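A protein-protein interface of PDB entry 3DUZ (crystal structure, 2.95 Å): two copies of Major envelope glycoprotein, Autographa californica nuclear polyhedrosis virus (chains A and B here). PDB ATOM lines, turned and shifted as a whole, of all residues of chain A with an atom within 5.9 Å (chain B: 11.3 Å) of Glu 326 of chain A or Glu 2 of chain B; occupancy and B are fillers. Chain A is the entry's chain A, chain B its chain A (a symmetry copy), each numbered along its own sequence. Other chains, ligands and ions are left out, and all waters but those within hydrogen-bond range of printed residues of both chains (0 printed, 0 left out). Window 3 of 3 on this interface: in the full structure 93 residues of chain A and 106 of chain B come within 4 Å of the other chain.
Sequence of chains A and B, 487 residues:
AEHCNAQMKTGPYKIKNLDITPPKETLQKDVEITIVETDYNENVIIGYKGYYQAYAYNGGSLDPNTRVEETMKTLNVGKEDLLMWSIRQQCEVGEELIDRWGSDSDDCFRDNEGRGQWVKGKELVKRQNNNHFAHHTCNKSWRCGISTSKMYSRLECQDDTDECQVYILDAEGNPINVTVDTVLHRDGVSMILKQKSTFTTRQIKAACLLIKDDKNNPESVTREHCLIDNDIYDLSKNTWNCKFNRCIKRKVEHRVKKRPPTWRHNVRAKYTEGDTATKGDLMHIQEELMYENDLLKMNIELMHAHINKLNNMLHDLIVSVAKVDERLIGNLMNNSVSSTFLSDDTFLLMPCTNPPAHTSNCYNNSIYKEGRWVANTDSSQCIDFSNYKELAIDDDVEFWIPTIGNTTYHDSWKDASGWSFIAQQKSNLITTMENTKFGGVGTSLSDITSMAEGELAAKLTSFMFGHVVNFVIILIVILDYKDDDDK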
ATOM      1  N   VAL A 321       0.183  -4.964  16.954  1.00  0.00           N
ATOM      2  CA  VAL A 321      -0.697  -3.939  17.498  1.00  0.00           C
ATOM      3  C   VAL A 321      -2.126  -4.464  17.729  1.00  0.00           C
ATOM      4  O   VAL A 321      -2.932  -3.827  18.410  1.00  0.00           O
ATOM      5  CB  VAL A 321      -0.658  -2.639  16.633  1.00  0.00           C
ATOM      6  CG1 VAL A 321      -1.617  -2.721  15.462  1.00  0.00           C
ATOM      7  CG2 VAL A 321      -0.930  -1.401  17.485  1.00  0.00           C
ATOM      8  N   ALA A 322      -2.428  -5.636  17.172  1.00  0.00           N
ATOM      9  CA  ALA A 322      -3.747  -6.244  17.335  1.00  0.00           C
ATOM     10  C   ALA A 322      -3.891  -6.888  18.707  1.00  0.00           C
ATOM     11  O   ALA A 322      -5.003  -7.057  19.197  1.00  0.00           O
ATOM     12  CB  ALA A 322      -4.015  -7.257  16.239  1.00  0.00           C
ATOM     13  N   LYS A 323      -2.766  -7.245  19.320  1.00  0.00           N
ATOM     14  CA  LYS A 323      -2.759  -7.807  20.665  1.00  0.00           C
ATOM     15  C   LYS A 323      -3.284  -6.800  21.674  1.00  0.00           C
ATOM     16  O   LYS A 323      -3.781  -7.186  22.727  1.00  0.00           O
ATOM     17  CB  LYS A 323      -1.351  -8.237  21.067  1.00  0.00           C
ATOM     18  CG  LYS A 323      -0.864  -9.482  20.377  1.00  0.00           C
ATOM     19  CD  LYS A 323       0.642  -9.475  20.294  1.00  0.00           C
ATOM     20  CE  LYS A 323       1.105 -10.456  19.244  1.00  0.00           C
ATOM     21  NZ  LYS A 323       2.531 -10.241  18.892  1.00  0.00           N
ATOM     22  N   VAL A 324      -3.154  -5.514  21.354  1.00  0.00           N
ATOM     23  CA  VAL A 324      -3.688  -4.447  22.205  1.00  0.00           C
ATOM     24  C   VAL A 324      -5.049  -3.990  21.674  1.00  0.00           C
ATOM     25  O   VAL A 324      -5.947  -3.665  22.450  1.00  0.00           O
ATOM     26  CB  VAL A 324      -2.682  -3.234  22.409  1.00  0.00           C
ATOM     27  CG1 VAL A 324      -1.238  -3.728  22.613  1.00  0.00           C
ATOM     28  CG2 VAL A 324      -2.741  -2.208  21.263  1.00  0.00           C
ATOM     29  N   ASP A 325      -5.201  -4.001  20.352  1.00  0.00           N
ATOM     30  CA  ASP A 325      -6.420  -3.524  19.707  1.00  0.00           C
ATOM     31  C   ASP A 325      -7.227  -4.670  19.105  1.00  0.00           C
ATOM     32  O   ASP A 325      -6.935  -5.156  18.013  1.00  0.00           O
ATOM     33  CB  ASP A 325      -6.094  -2.474  18.644  1.00  0.00           C
ATOM     34  CG  ASP A 325      -7.329  -1.768  18.122  1.00  0.00           C
ATOM     35  OD1 ASP A 325      -8.374  -2.429  17.934  1.00  0.00           O
ATOM     36  OD2 ASP A 325      -7.251  -0.544  17.892  1.00  0.00           O
ATOM     37  N   GLU A 326      -8.266  -5.067  19.826  1.00  0.00           N
ATOM     38  CA  GLU A 326      -9.085  -6.222  19.473  1.00  0.00           C
ATOM     39  C   GLU A 326      -9.996  -6.003  18.256  1.00  0.00           C
ATOM     40  O   GLU A 326     -10.472  -6.967  17.657  1.00  0.00           O
ATOM     41  CB  GLU A 326      -9.925  -6.634  20.682  1.00  0.00           C
ATOM     42  CG  GLU A 326      -9.284  -6.269  22.015  1.00  0.00           C
ATOM     43  CD  GLU A 326      -9.920  -6.974  23.199  1.00  0.00           C
ATOM     44  OE1 GLU A 326     -11.171  -7.043  23.264  1.00  0.00           O
ATOM     45  OE2 GLU A 326      -9.157  -7.451  24.072  1.00  0.00           O
ATOM     46  N   ARG A 327     -10.228  -4.743  17.893  1.00  0.00           N
ATOM     47  CA  ARG A 327     -11.174  -4.410  16.815  1.00  0.00           C
ATOM     48  C   ARG A 327     -10.504  -3.994  15.505  1.00  0.00           C
ATOM     49  O   ARG A 327     -11.189  -3.695  14.519  1.00  0.00           O
ATOM     50  CB  ARG A 327     -12.145  -3.319  17.268  1.00  0.00           C
ATOM     51  CG  ARG A 327     -12.920  -3.667  18.520  1.00  0.00           C
ATOM     52  CD  ARG A 327     -14.264  -2.989  18.507  1.00  0.00           C
ATOM     53  NE  ARG A 327     -15.243  -3.773  17.755  1.00  0.00           N
ATOM     54  CZ  ARG A 327     -16.096  -3.265  16.865  1.00  0.00           C
ATOM     55  NH1 ARG A 327     -16.089  -1.963  16.585  1.00  0.00           N
ATOM     56  NH2 ARG A 327     -16.950  -4.068  16.239  1.00  0.00           N
ATOM     57  N   LEU A 328      -9.173  -3.992  15.507  1.00  0.00           N
ATOM     58  CA  LEU A 328      -8.377  -3.494  14.387  1.00  0.00           C
ATOM     59  C   LEU A 328      -8.548  -4.322  13.125  1.00  0.00           C
ATOM     60  O   LEU A 328      -8.793  -3.781  12.045  1.00  0.00           O
ATOM     61  CB  LEU A 328      -6.893  -3.441  14.763  1.00  0.00           C
ATOM     62  CG  LEU A 328      -5.909  -3.196  13.616  1.00  0.00           C
ATOM     63  CD1 LEU A 328      -5.930  -1.737  13.166  1.00  0.00           C
ATOM     64  CD2 LEU A 328      -4.512  -3.626  14.021  1.00  0.00           C
ATOM     65  N   ILE A 329      -8.403  -5.635  13.271  1.00  0.00           N
ATOM     66  CA  ILE A 329      -8.490  -6.542  12.141  1.00  0.00           C
ATOM     67  C   ILE A 329      -9.850  -6.372  11.472  1.00  0.00           C
ATOM     68  O   ILE A 329      -9.956  -6.388  10.247  1.00  0.00           O
ATOM     69  CB  ILE A 329      -8.217  -7.997  12.576  1.00  0.00           C
ATOM     70  CG1 ILE A 329      -6.772  -8.119  13.083  1.00  0.00           C
ATOM     71  CG2 ILE A 329      -8.468  -8.965  11.425  1.00  0.00           C
ATOM     72  CD1 ILE A 329      -6.432  -9.435  13.775  1.00  0.00           C
ATOM     73  N   GLY A 330     -10.874  -6.166  12.291  1.00  0.00           N
ATOM     74  CA  GLY A 330     -12.202  -5.840  11.800  1.00  0.00           C
ATOM     75  C   GLY A 330     -12.218  -4.596  10.935  1.00  0.00           C
ATOM     76  O   GLY A 330     -12.825  -4.592   9.865  1.00  0.00           O
ATOM     77  N   VAL A 337     -15.411  -7.170  13.738  1.00  0.00           N
ATOM     78  CA  VAL A 337     -15.028  -8.421  14.413  1.00  0.00           C
ATOM     79  C   VAL A 337     -13.915  -8.221  15.449  1.00  0.00           C
ATOM     80  O   VAL A 337     -12.997  -7.426  15.250  1.00  0.00           O
ATOM     81  CB  VAL A 337     -14.627  -9.567  13.416  1.00  0.00           C
ATOM     82  CG1 VAL A 337     -15.852 -10.188  12.761  1.00  0.00           C
ATOM     83  CG2 VAL A 337     -13.641  -9.087  12.362  1.00  0.00           C
ATOM     84  N   SER A 338     -14.008  -8.961  16.550  1.00  0.00           N
ATOM     85  CA  SER A 338     -13.053  -8.860  17.651  1.00  0.00           C
ATOM     86  C   SER A 338     -12.072 -10.034  17.662  1.00  0.00           C
ATOM     87  O   SER A 338     -12.466 -11.189  17.507  1.00  0.00           O
ATOM     88  CB  SER A 338     -13.798  -8.750  18.986  1.00  0.00           C
ATOM     89  OG  SER A 338     -13.070  -9.339  20.047  1.00  0.00           O
ATOM     90  N   SER A 339     -10.794  -9.723  17.856  1.00  0.00           N
ATOM     91  CA  SER A 339      -9.727 -10.717  17.763  1.00  0.00           C
ATOM     92  C   SER A 339      -9.210 -11.159  19.131  1.00  0.00           C
ATOM     93  O   SER A 339      -9.059 -10.338  20.037  1.00  0.00           O
ATOM     94  CB  SER A 339      -8.573 -10.178  16.908  1.00  0.00           C
ATOM     95  OG  SER A 339      -8.112  -8.926  17.392  1.00  0.00           O
ATOM     96  N   CYS A 352     -19.355  -8.929  15.376  1.00  0.00           N
ATOM     97  CA  CYS A 352     -19.834  -7.746  16.115  1.00  0.00           C
ATOM     98  C   CYS A 352     -20.608  -6.790  15.199  1.00  0.00           C
ATOM     99  O   CYS A 352     -20.440  -6.828  13.979  1.00  0.00           O
ATOM    100  CB  CYS A 352     -18.653  -6.963  16.701  1.00  0.00           C
ATOM    101  SG  CYS A 352     -17.781  -7.714  18.083  1.00  0.00           S
ATOM    102  N   ASN A 354     -22.012  -2.433  15.910  1.00  0.00           N
ATOM    103  CA  ASN A 354     -22.078  -1.375  16.916  1.00  0.00           C
ATOM    104  C   ASN A 354     -23.016  -0.215  16.561  1.00  0.00           C
ATOM    105  O   ASN A 354     -23.325  -0.012  15.382  1.00  0.00           O
ATOM    106  CB  ASN A 354     -20.666  -0.838  17.185  1.00  0.00           C
ATOM    107  CG  ASN A 354     -19.733  -1.894  17.763  1.00  0.00           C
ATOM    108  OD1 ASN A 354     -20.018  -3.092  17.723  1.00  0.00           O
ATOM    109  ND2 ASN A 354     -18.608  -1.446  18.304  1.00  0.00           N
ATOM    110  N   GLU B   2     -17.233  -3.705  20.974  1.00  0.00           N
ATOM    111  CA  GLU B   2     -16.791  -4.808  21.871  1.00  0.00           C
ATOM    112  C   GLU B   2     -17.965  -5.462  22.633  1.00  0.00           C
ATOM    113  O   GLU B   2     -17.979  -5.507  23.870  1.00  0.00           O
ATOM    114  CB  GLU B   2     -15.719  -4.302  22.841  1.00  0.00           C
ATOM    115  CG  GLU B   2     -14.881  -5.401  23.487  1.00  0.00           C
ATOM    116  CD  GLU B   2     -14.625  -5.149  24.963  1.00  0.00           C
ATOM    117  OE1 GLU B   2     -14.837  -4.008  25.432  1.00  0.00           O
ATOM    118  OE2 GLU B   2     -14.214  -6.101  25.662  1.00  0.00           O
ATOM    119  N   HIS B   3     -18.952  -5.946  21.879  1.00  0.00           N
ATOM    120  CA  HIS B   3     -19.968  -6.869  22.402  1.00  0.00           C
ATOM    121  C   HIS B   3     -20.301  -7.930  21.344  1.00  0.00           C
ATOM    122  O   HIS B   3     -20.994  -7.653  20.358  1.00  0.00           O
ATOM    123  CB  HIS B   3     -21.225  -6.134  22.882  1.00  0.00           C
ATOM    124  CG  HIS B   3     -22.043  -6.930  23.852  1.00  0.00           C
ATOM    125  ND1 HIS B   3     -21.786  -6.937  25.211  1.00  0.00           N
ATOM    126  CD2 HIS B   3     -23.093  -7.768  23.659  1.00  0.00           C
ATOM    127  CE1 HIS B   3     -22.650  -7.735  25.814  1.00  0.00           C
ATOM    128  NE2 HIS B   3     -23.455  -8.250  24.895  1.00  0.00           N
ATOM    129  N   CYS B   4     -19.800  -9.145  21.570  1.00  0.00           N
ATOM    130  CA  CYS B   4     -19.702 -10.164  20.523  1.00  0.00           C
ATOM    131  C   CYS B   4     -20.319 -11.507  20.892  1.00  0.00           C
ATOM    132  O   CYS B   4     -20.286 -11.920  22.051  1.00  0.00           O
ATOM    133  CB  CYS B   4     -18.230 -10.377  20.162  1.00  0.00           C
ATOM    134  SG  CYS B   4     -17.355  -8.844  19.736  1.00  0.00           S
ATOM    135  N   ASN B   5     -20.873 -12.183  19.887  1.00  0.00           N
ATOM    136  CA  ASN B   5     -21.335 -13.559  20.020  1.00  0.00           C
ATOM    137  C   ASN B   5     -20.127 -14.470  20.252  1.00  0.00           C
ATOM    138  O   ASN B   5     -19.322 -14.693  19.343  1.00  0.00           O
ATOM    139  CB  ASN B   5     -22.117 -13.973  18.762  1.00  0.00           C
ATOM    140  CG  ASN B   5     -22.644 -15.407  18.822  1.00  0.00           C
ATOM    141  OD1 ASN B   5     -21.930 -16.341  19.193  1.00  0.00           O
ATOM    142  ND2 ASN B   5     -23.900 -15.587  18.422  1.00  0.00           N
ATOM    143  N   ALA B   6     -19.998 -14.976  21.477  1.00  0.00           N
ATOM    144  CA  ALA B   6     -18.895 -15.867  21.838  1.00  0.00           C
ATOM    145  C   ALA B   6     -19.077 -17.271  21.258  1.00  0.00           C
ATOM    146  O   ALA B   6     -18.096 -17.975  21.002  1.00  0.00           O
ATOM    147  CB  ALA B   6     -18.736 -15.928  23.348  1.00  0.00           C
ATOM    148  N   LYS B   9     -16.919 -18.278  17.656  1.00  0.00           N
ATOM    149  CA  LYS B   9     -15.478 -18.121  17.446  1.00  0.00           C
ATOM    150  C   LYS B   9     -15.006 -18.950  16.256  1.00  0.00           C
ATOM    151  O   LYS B   9     -15.104 -20.176  16.271  1.00  0.00           O
ATOM    152  CB  LYS B   9     -14.694 -18.541  18.694  1.00  0.00           C
ATOM    153  CG  LYS B   9     -14.778 -17.591  19.882  1.00  0.00           C
ATOM    154  CD  LYS B   9     -14.003 -18.160  21.066  1.00  0.00           C
ATOM    155  CE  LYS B   9     -14.272 -17.385  22.346  1.00  0.00           C
ATOM    156  NZ  LYS B   9     -13.706 -18.075  23.544  1.00  0.00           N
ATOM    157  N   ASP B 316      -5.598   3.077   8.975  1.00  0.00           N
ATOM    158  CA  ASP B 316      -6.267   2.314  10.022  1.00  0.00           C
ATOM    159  C   ASP B 316      -5.280   1.941  11.127  1.00  0.00           C
ATOM    160  O   ASP B 316      -5.615   2.018  12.308  1.00  0.00           O
ATOM    161  CB  ASP B 316      -6.939   1.068   9.437  1.00  0.00           C
ATOM    162  CG  ASP B 316      -8.023   1.404   8.421  1.00  0.00           C
ATOM    163  OD1 ASP B 316      -8.187   2.598   8.100  1.00  0.00           O
ATOM    164  OD2 ASP B 316      -8.716   0.479   7.937  1.00  0.00           O
ATOM    165  N   LEU B 317      -4.064   1.550  10.732  1.00  0.00           N
ATOM    166  CA  LEU B 317      -2.964   1.341  11.678  1.00  0.00           C
ATOM    167  C   LEU B 317      -2.721   2.578  12.521  1.00  0.00           C
ATOM    168  O   LEU B 317      -2.791   2.514  13.745  1.00  0.00           O
ATOM    169  CB  LEU B 317      -1.669   0.959  10.954  1.00  0.00           C
ATOM    170  CG  LEU B 317      -1.074  -0.451  11.065  1.00  0.00           C
ATOM    171  CD1 LEU B 317      -0.506  -0.716  12.437  1.00  0.00           C
ATOM    172  CD2 LEU B 317      -2.086  -1.512  10.707  1.00  0.00           C
ATOM    173  N   VAL B 319      -4.486   5.448  13.255  1.00  0.00           N
ATOM    174  CA  VAL B 319      -5.546   5.807  14.215  1.00  0.00           C
ATOM    175  C   VAL B 319      -5.537   4.935  15.471  1.00  0.00           C
ATOM    176  O   VAL B 319      -5.737   5.434  16.578  1.00  0.00           O
ATOM    177  CB  VAL B 319      -6.991   5.825  13.600  1.00  0.00           C
ATOM    178  CG1 VAL B 319      -7.182   7.010  12.665  1.00  0.00           C
ATOM    179  CG2 VAL B 319      -7.340   4.510  12.906  1.00  0.00           C
ATOM    180  N   SER B 320      -5.289   3.639  15.286  1.00  0.00           N
ATOM    181  CA  SER B 320      -5.255   2.679  16.384  1.00  0.00           C
ATOM    182  C   SER B 320      -4.083   2.944  17.326  1.00  0.00           C
ATOM    183  O   SER B 320      -4.270   3.074  18.537  1.00  0.00           O
ATOM    184  CB  SER B 320      -5.193   1.251  15.842  1.00  0.00           C
ATOM    185  OG  SER B 320      -4.777   0.342  16.846  1.00  0.00           O
ATOM    186  N   VAL B 321      -2.882   3.037  16.769  1.00  0.00           N
ATOM    187  CA  VAL B 321      -1.683   3.181  17.583  1.00  0.00           C
ATOM    188  C   VAL B 321      -1.507   4.620  18.106  1.00  0.00           C
ATOM    189  O   VAL B 321      -0.702   4.871  19.005  1.00  0.00           O
ATOM    190  CB  VAL B 321      -0.420   2.648  16.835  1.00  0.00           C
ATOM    191  CG1 VAL B 321       0.175   3.702  15.922  1.00  0.00           C
ATOM    192  CG2 VAL B 321       0.621   2.117  17.819  1.00  0.00           C
ATOM    193  N   LYS B 323      -3.899   6.281  19.587  1.00  0.00           N
ATOM    194  CA  LYS B 323      -4.633   6.327  20.846  1.00  0.00           C
ATOM    195  C   LYS B 323      -3.702   6.101  22.024  1.00  0.00           C
ATOM    196  O   LYS B 323      -3.994   6.537  23.132  1.00  0.00           O
ATOM    197  CB  LYS B 323      -5.740   5.276  20.868  1.00  0.00           C
ATOM    198  CG  LYS B 323      -6.917   5.600  19.989  1.00  0.00           C
ATOM    199  CD  LYS B 323      -7.604   4.329  19.553  1.00  0.00           C
ATOM    200  CE  LYS B 323      -8.476   4.603  18.351  1.00  0.00           C
ATOM    201  NZ  LYS B 323      -8.897   3.343  17.688  1.00  0.00           N
ATOM    202  N   VAL B 324      -2.593   5.403  21.782  1.00  0.00           N
ATOM    203  CA  VAL B 324      -1.577   5.181  22.813  1.00  0.00           C
ATOM    204  C   VAL B 324      -0.445   6.200  22.657  1.00  0.00           C
ATOM    205  O   VAL B 324       0.115   6.670  23.646  1.00  0.00           O
ATOM    206  CB  VAL B 324      -1.039   3.687  22.864  1.00  0.00           C
ATOM    207  CG1 VAL B 324      -2.182   2.671  22.681  1.00  0.00           C
ATOM    208  CG2 VAL B 324       0.084   3.419  21.846  1.00  0.00           C
ATOM    209  N   ASP B 344     -12.841   6.429  18.021  1.00  0.00           N
ATOM    210  CA  ASP B 344     -11.693   5.682  17.506  1.00  0.00           C
ATOM    211  C   ASP B 344     -11.240   6.373  16.238  1.00  0.00           C
ATOM    212  O   ASP B 344     -10.067   6.333  15.863  1.00  0.00           O
ATOM    213  CB  ASP B 344     -12.089   4.248  17.157  1.00  0.00           C
ATOM    214  CG  ASP B 344     -13.132   3.687  18.096  1.00  0.00           C
ATOM    215  OD1 ASP B 344     -12.754   3.205  19.181  1.00  0.00           O
ATOM    216  OD2 ASP B 344     -14.330   3.726  17.739  1.00  0.00           O
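SG of Cys 352 of chain A is disulfide-bonded to SG of Cys 4 of chain B (2.0 Å). The side-chain hydroxyl (OG) of Ser 320 of chain B lies within hydrogen-bond range of the side-chain carboxylate (OD2) of Asp 325 of chain A (2.8 Å).
N of Ser 339 of chain A lies within hydrogen-bond range of O of Glu 326 of chain A, 2.8 Å away. The guanidinium group of Arg 327 of chain A sits close to the side-chain amide nitrogen of Asn 354 of chain A, 3.1 Å away. The backbone NH (N) of Leu 328 of chain A lies within hydrogen-bond range of the side-chain carboxylate (OD1) of Asp 325 of chain A (3.0 Å). OD1 of Asp 325 of chain A is in hydrogen-bond range of N of Arg 327 of chain A (3.0 Å).
CG1 of Val 321 of chain A touches CD1 of Leu 317 of chain B, at 3.8 Å. CG2 of Val 321 of chain A touches CG2 of Val 321 of chain B, 3.9 Å away. Glu 326 of chain A touches Glu 2 of chain B. Arg 327 of chain A touches Glu 2 of chain B (NE to N, 3.8 Å). O of Asp 316 of chain B touches CD1 of Leu 328 of chain A (3.9 Å). Cys 4 of chain B touches Ser 338 of chain A. Cys 352 of chain A touches His 3 of chain B (SG to O, 3.9 Å). Asn 354 of chain A touches Glu 2 of chain B.
Printed residues of chain B within 4 Å of Glu 326 of chain A: Glu 2. Printed residues of chain A within 4 Å of Glu 2 of chain B: Glu 326 (3.99 Å), Arg 327 (3.8 Å) and Asn 354 (3.8 Å). No residue of chain B comes within 4 Å of Ala 322 of chain A. Of chain B, only Glu 2 comes within 4 Å of Arg 327 of chain A. Ser 338 of chain A touches just one residue of chain B: Cys 4. No residue of chain B comes within 4 Å of Ser 339 of chain A. Of the printed residues of chain A, His 3 of chain B touches Cys 352 (3.9 Å). Of the printed residues of chain A, Ser 320 of chain B touches Asp 325 (2.8 Å). Of the printed residues of chain A, Cys 4 of chain B touches Ser 338 (3.6 Å) and Cys 352 (2.0 Å). The nearest printed residue of chain B that does not touch Glu 326 of chain A is Ser 320 of chain B (7.1 Å).
Printed residues of chain B that touch a printed residue of chain A: Glu 2, His 3, Cys 4, Asp 316, Leu 317, Ser 320 and Val 321. Hydrophobic or aromatic side chains of chain A within 4 Å of the printed part of chain B: Val 321 and Leu 328. Among the printed residues, no Asp or Glu carboxylate lies within 4 Å of a Lys or Arg side-chain nitrogen of the other chain.
Val 321 of chain A touches its own counterpart, Val 321 of chain B. 3 positions are printed for both chains. Of the 10 pairs that touch across the chains among the printed residues, 1 has its exchanged pair printed and touching as well.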
